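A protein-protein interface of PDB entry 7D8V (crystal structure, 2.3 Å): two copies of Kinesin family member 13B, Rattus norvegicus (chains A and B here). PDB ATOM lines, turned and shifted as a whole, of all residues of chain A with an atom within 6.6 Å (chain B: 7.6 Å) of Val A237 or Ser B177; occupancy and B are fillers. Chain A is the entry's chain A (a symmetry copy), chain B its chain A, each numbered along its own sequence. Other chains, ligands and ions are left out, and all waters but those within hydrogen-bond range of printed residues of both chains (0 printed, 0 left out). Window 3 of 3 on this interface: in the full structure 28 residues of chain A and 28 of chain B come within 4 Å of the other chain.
Val A237 touches just one residue of chain B: Ser B177 (2.6 Å).
Ser B177 touches just these residues of chain A: Val A237 and Gly A240.
Printed residues of chain A within 4 Å of Leu B179: Tyr A235 (3.7 Å).
Printed residues of chain B within 4 Å of Tyr A235: His B176 (3.7 Å), Val B178 (3.8 Å) and Leu B179 (3.7 Å).
Printed residues of chain B within 4 Å of Thr A241: Val B178.
Of the printed residues of chain B, Gly A240 touches Ser B177 (3.8 Å) and Val B178 (3.8 Å).
The nearest residue of chain A that does not touch Ser B177 is Asp A236 (4.5 Å).
A ring nitrogen (ND1) of His B176 lies close to the backbone NH (N) of Val B178 (3.3 Å).
A ring nitrogen (ND1) of His B176 is in hydrogen-bond range of the backbone NH of Leu B179.
The backbone carbonyl oxygen of Glu A141 lies within hydrogen-bond range of the backbone NH of Tyr A235 (2.7 Å).
N of Asp A236 is in hydrogen-bond range of O of Thr A241.
OG1 of Thr A241 is in hydrogen-bond range of OG of Ser A239, 2.6 Å away.
Hydrophobic or aromatic side chains of chain A that line the printed part of chain B: Tyr A235 and Val A237.
Of the 8 printed residues of chain B, 4 touch a printed residue of chain A.
Printed residues of chain B that touch a printed residue of chain A: His B176, Ser B177, Val B178 and Leu B179.
Among the printed residues, 8 pairs touch across the chains.
Among the printed residues, no Asp or Glu carboxylate lies within 4 Å of a Lys or Arg side-chain nitrogen of the other chain.
Tyr A235 touches His B176 (CG to CE1, 3.7 Å).
Tyr A235 touches Val B178.
Tyr A235 touches Leu B179 (CE2 to CD2, 3.7 Å).
Gly A240 touches Ser B177.
C of Gly A240 touches CG2 of Val B178 (3.8 Å).
Thr A241 touches Val B178.
NE2 of His B176 lies within hydrogen-bond range of O of Glu A140, at 2.8 Å.
OG of Ser B177 is in hydrogen-bond range of O of Val A237 (2.6 Å).
No position is printed for both chains.
Of the 8 pairs that touch across the chains among the printed residues, none has its exchanged pair printed and touching as well.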
ATOM      1  N   GLU A 140      26.105  -4.548   7.340  1.00  0.00           N
ATOM      2  CA  GLU A 140      25.454  -4.376   6.054  1.00  0.00           C
ATOM      3  C   GLU A 140      24.878  -5.662   5.491  1.00  0.00           C
ATOM      4  O   GLU A 140      24.128  -5.613   4.511  1.00  0.00           O
ATOM      5  CB  GLU A 140      26.436  -3.745   5.077  1.00  0.00           C
ATOM      6  CG  GLU A 140      27.627  -4.646   4.831  1.00  0.00           C
ATOM      7  CD  GLU A 140      28.695  -3.997   3.950  1.00  0.00           C
ATOM      8  OE1 GLU A 140      28.445  -2.995   3.228  1.00  0.00           O
ATOM      9  OE2 GLU A 140      29.815  -4.534   3.958  1.00  0.00           O
ATOM     10  N   GLU A 141      25.198  -6.801   6.091  1.00  0.00           N
ATOM     11  CA  GLU A 141      24.549  -8.057   5.758  1.00  0.00           C
ATOM     12  C   GLU A 141      23.385  -8.397   6.676  1.00  0.00           C
ATOM     13  O   GLU A 141      22.670  -9.359   6.385  1.00  0.00           O
ATOM     14  CB  GLU A 141      25.566  -9.202   5.800  1.00  0.00           C
ATOM     15  CG  GLU A 141      26.678  -9.132   4.757  1.00  0.00           C
ATOM     16  CD  GLU A 141      27.366 -10.478   4.616  1.00  0.00           C
ATOM     17  OE1 GLU A 141      26.798 -11.473   5.128  1.00  0.00           O
ATOM     18  OE2 GLU A 141      28.442 -10.555   3.994  1.00  0.00           O
ATOM     19  N   TYR A 235      20.731  -9.703   4.482  1.00  0.00           N
ATOM     20  CA  TYR A 235      20.856  -9.104   3.159  1.00  0.00           C
ATOM     21  C   TYR A 235      21.830  -9.924   2.321  1.00  0.00           C
ATOM     22  O   TYR A 235      23.007 -10.036   2.666  1.00  0.00           O
ATOM     23  CB  TYR A 235      21.298  -7.638   3.245  1.00  0.00           C
ATOM     24  CG  TYR A 235      20.354  -6.773   4.050  1.00  0.00           C
ATOM     25  CD1 TYR A 235      20.587  -6.533   5.404  1.00  0.00           C
ATOM     26  CD2 TYR A 235      19.218  -6.218   3.466  1.00  0.00           C
ATOM     27  CE1 TYR A 235      19.718  -5.748   6.152  1.00  0.00           C
ATOM     28  CE2 TYR A 235      18.341  -5.442   4.201  1.00  0.00           C
ATOM     29  CZ  TYR A 235      18.595  -5.210   5.551  1.00  0.00           C
ATOM     30  OH  TYR A 235      17.737  -4.435   6.312  1.00  0.00           O
ATOM     31  N   ASP A 236      21.306 -10.524   1.255  1.00  0.00           N
ATOM     32  CA  ASP A 236      22.019 -11.211   0.184  1.00  0.00           C
ATOM     33  C   ASP A 236      22.500 -10.132  -0.782  1.00  0.00           C
ATOM     34  O   ASP A 236      21.838  -9.791  -1.771  1.00  0.00           O
ATOM     35  CB  ASP A 236      21.064 -12.179  -0.504  1.00  0.00           C
ATOM     36  CG  ASP A 236      21.764 -13.217  -1.345  1.00  0.00           C
ATOM     37  OD1 ASP A 236      21.166 -14.290  -1.551  1.00  0.00           O
ATOM     38  OD2 ASP A 236      22.913 -13.002  -1.751  1.00  0.00           O
ATOM     39  N   VAL A 237      23.665  -9.562  -0.462  1.00  0.00           N
ATOM     40  CA  VAL A 237      24.055  -8.311  -1.102  1.00  0.00           C
ATOM     41  C   VAL A 237      24.509  -8.528  -2.537  1.00  0.00           C
ATOM     42  O   VAL A 237      24.298  -7.660  -3.392  1.00  0.00           O
ATOM     43  CB  VAL A 237      25.133  -7.581  -0.272  1.00  0.00           C
ATOM     44  CG1 VAL A 237      24.766  -7.603   1.208  1.00  0.00           C
ATOM     45  CG2 VAL A 237      26.545  -8.164  -0.519  1.00  0.00           C
ATOM     46  N   LYS A 238      25.140  -9.659  -2.843  1.00  0.00           N
ATOM     47  CA  LYS A 238      25.506  -9.843  -4.239  1.00  0.00           C
ATOM     48  C   LYS A 238      24.334 -10.320  -5.091  1.00  0.00           C
ATOM     49  O   LYS A 238      24.404 -10.239  -6.312  1.00  0.00           O
ATOM     50  CB  LYS A 238      26.717 -10.780  -4.368  1.00  0.00           C
ATOM     51  CG  LYS A 238      28.006 -10.256  -3.828  1.00  0.00           C
ATOM     52  CD  LYS A 238      29.121 -11.265  -3.984  1.00  0.00           C
ATOM     53  CE  LYS A 238      30.417 -10.704  -3.454  1.00  0.00           C
ATOM     54  NZ  LYS A 238      31.436 -11.755  -3.623  1.00  0.00           N
ATOM     55  N   SER A 239      23.237 -10.770  -4.499  1.00  0.00           N
ATOM     56  CA  SER A 239      22.051 -11.003  -5.309  1.00  0.00           C
ATOM     57  C   SER A 239      21.023  -9.880  -5.183  1.00  0.00           C
ATOM     58  O   SER A 239      20.000  -9.917  -5.879  1.00  0.00           O
ATOM     59  CB  SER A 239      21.416 -12.356  -4.958  1.00  0.00           C
ATOM     60  OG  SER A 239      20.340 -12.190  -4.067  1.00  0.00           O
ATOM     61  N   GLY A 240      21.287  -8.876  -4.340  1.00  0.00           N
ATOM     62  CA  GLY A 240      20.375  -7.761  -4.166  1.00  0.00           C
ATOM     63  C   GLY A 240      19.061  -8.150  -3.538  1.00  0.00           C
ATOM     64  O   GLY A 240      18.027  -7.550  -3.851  1.00  0.00           O
ATOM     65  N   THR A 241      19.062  -9.156  -2.668  1.00  0.00           N
ATOM     66  CA  THR A 241      17.827  -9.620  -2.054  1.00  0.00           C
ATOM     67  C   THR A 241      18.006  -9.694  -0.545  1.00  0.00           C
ATOM     68  O   THR A 241      19.107  -9.545  -0.021  1.00  0.00           O
ATOM     69  CB  THR A 241      17.406 -10.985  -2.614  1.00  0.00           C
ATOM     70  OG1 THR A 241      18.441 -11.949  -2.362  1.00  0.00           O
ATOM     71  CG2 THR A 241      17.118 -10.888  -4.137  1.00  0.00           C
ATOM     72  N   GLU B 175      25.641   3.607   0.028  1.00  0.00           N
ATOM     73  CA  GLU B 175      24.884   2.851  -0.955  1.00  0.00           C
ATOM     74  C   GLU B 175      24.798   1.392  -0.521  1.00  0.00           C
ATOM     75  O   GLU B 175      25.736   0.845   0.071  1.00  0.00           O
ATOM     76  CB  GLU B 175      25.506   2.960  -2.349  1.00  0.00           C
ATOM     77  CG  GLU B 175      26.916   2.419  -2.437  1.00  0.00           C
ATOM     78  CD  GLU B 175      27.535   2.681  -3.795  1.00  0.00           C
ATOM     79  OE1 GLU B 175      26.841   3.293  -4.640  1.00  0.00           O
ATOM     80  OE2 GLU B 175      28.703   2.278  -4.023  1.00  0.00           O
ATOM     81  N   HIS B 176      23.654   0.778  -0.798  1.00  0.00           N
ATOM     82  CA  HIS B 176      23.383  -0.594  -0.406  1.00  0.00           C
ATOM     83  C   HIS B 176      22.689  -1.299  -1.561  1.00  0.00           C
ATOM     84  O   HIS B 176      21.694  -0.793  -2.090  1.00  0.00           O
ATOM     85  CB  HIS B 176      22.506  -0.645   0.856  1.00  0.00           C
ATOM     86  CG  HIS B 176      22.554  -1.960   1.567  1.00  0.00           C
ATOM     87  ND1 HIS B 176      21.525  -2.878   1.504  1.00  0.00           N
ATOM     88  CD2 HIS B 176      23.509  -2.518   2.346  1.00  0.00           C
ATOM     89  CE1 HIS B 176      21.844  -3.944   2.215  1.00  0.00           C
ATOM     90  NE2 HIS B 176      23.044  -3.754   2.734  1.00  0.00           N
ATOM     91  N   SER B 177      23.194  -2.479  -1.926  1.00  0.00           N
ATOM     92  CA  SER B 177      22.638  -3.191  -3.074  1.00  0.00           C
ATOM     93  C   SER B 177      21.182  -3.596  -2.854  1.00  0.00           C
ATOM     94  O   SER B 177      20.421  -3.715  -3.822  1.00  0.00           O
ATOM     95  CB  SER B 177      23.485  -4.420  -3.392  1.00  0.00           C
ATOM     96  OG  SER B 177      23.021  -5.544  -2.679  1.00  0.00           O
ATOM     97  N   VAL B 178      20.764  -3.801  -1.607  1.00  0.00           N
ATOM     98  CA  VAL B 178      19.384  -4.150  -1.312  1.00  0.00           C
ATOM     99  C   VAL B 178      18.557  -2.924  -0.948  1.00  0.00           C
ATOM    100  O   VAL B 178      17.424  -2.781  -1.412  1.00  0.00           O
ATOM    101  CB  VAL B 178      19.309  -5.219  -0.193  1.00  0.00           C
ATOM    102  CG1 VAL B 178      17.924  -5.835  -0.153  1.00  0.00           C
ATOM    103  CG2 VAL B 178      20.341  -6.318  -0.417  1.00  0.00           C
ATOM    104  N   LEU B 179      19.091  -2.041  -0.100  1.00  0.00           N
ATOM    105  CA  LEU B 179      18.311  -0.910   0.386  1.00  0.00           C
ATOM    106  C   LEU B 179      18.383   0.324  -0.512  1.00  0.00           C
ATOM    107  O   LEU B 179      17.514   1.196  -0.409  1.00  0.00           O
ATOM    108  CB  LEU B 179      18.768  -0.529   1.798  1.00  0.00           C
ATOM    109  CG  LEU B 179      18.716  -1.659   2.831  1.00  0.00           C
ATOM    110  CD1 LEU B 179      19.339  -1.216   4.127  1.00  0.00           C
ATOM    111  CD2 LEU B 179      17.275  -2.135   3.053  1.00  0.00           C
ATOM    112  N   GLY B 180      19.397   0.430  -1.374  1.00  0.00           N
ATOM    113  CA  GLY B 180      19.636   1.652  -2.095  1.00  0.00           C
ATOM    114  C   GLY B 180      20.371   2.662  -1.236  1.00  0.00           C
ATOM    115  O   GLY B 180      20.881   2.342  -0.154  1.00  0.00           O
ATOM    116  N   PRO B 181      20.448   3.903  -1.710  1.00  0.00           N
ATOM    117  CA  PRO B 181      21.061   4.959  -0.896  1.00  0.00           C
ATOM    118  C   PRO B 181      20.307   5.119   0.413  1.00  0.00           C
ATOM    119  O   PRO B 181      19.076   5.217   0.433  1.00  0.00           O
ATOM    120  CB  PRO B 181      20.942   6.205  -1.778  1.00  0.00           C
ATOM    121  CG  PRO B 181      19.821   5.876  -2.760  1.00  0.00           C
ATOM    122  CD  PRO B 181      19.949   4.404  -3.003  1.00  0.00           C
ATOM    123  N   TYR B 182      21.051   5.120   1.514  1.00  0.00           N
ATOM    124  CA  TYR B 182      20.424   5.288   2.816  1.00  0.00           C
ATOM    125  C   TYR B 182      21.360   6.040   3.749  1.00  0.00           C
ATOM    126  O   TYR B 182      22.556   6.176   3.489  1.00  0.00           O
ATOM    127  CB  TYR B 182      20.038   3.938   3.422  1.00  0.00           C
ATOM    128  CG  TYR B 182      21.241   3.159   3.883  1.00  0.00           C
ATOM    129  CD1 TYR B 182      21.618   3.154   5.224  1.00  0.00           C
ATOM    130  CD2 TYR B 182      22.027   2.463   2.974  1.00  0.00           C
ATOM    131  CE1 TYR B 182      22.717   2.460   5.647  1.00  0.00           C
ATOM    132  CE2 TYR B 182      23.138   1.756   3.391  1.00  0.00           C
ATOM    133  CZ  TYR B 182      23.468   1.760   4.731  1.00  0.00           C
ATOM    134  OH  TYR B 182      24.560   1.081   5.166  1.00  0.00           O
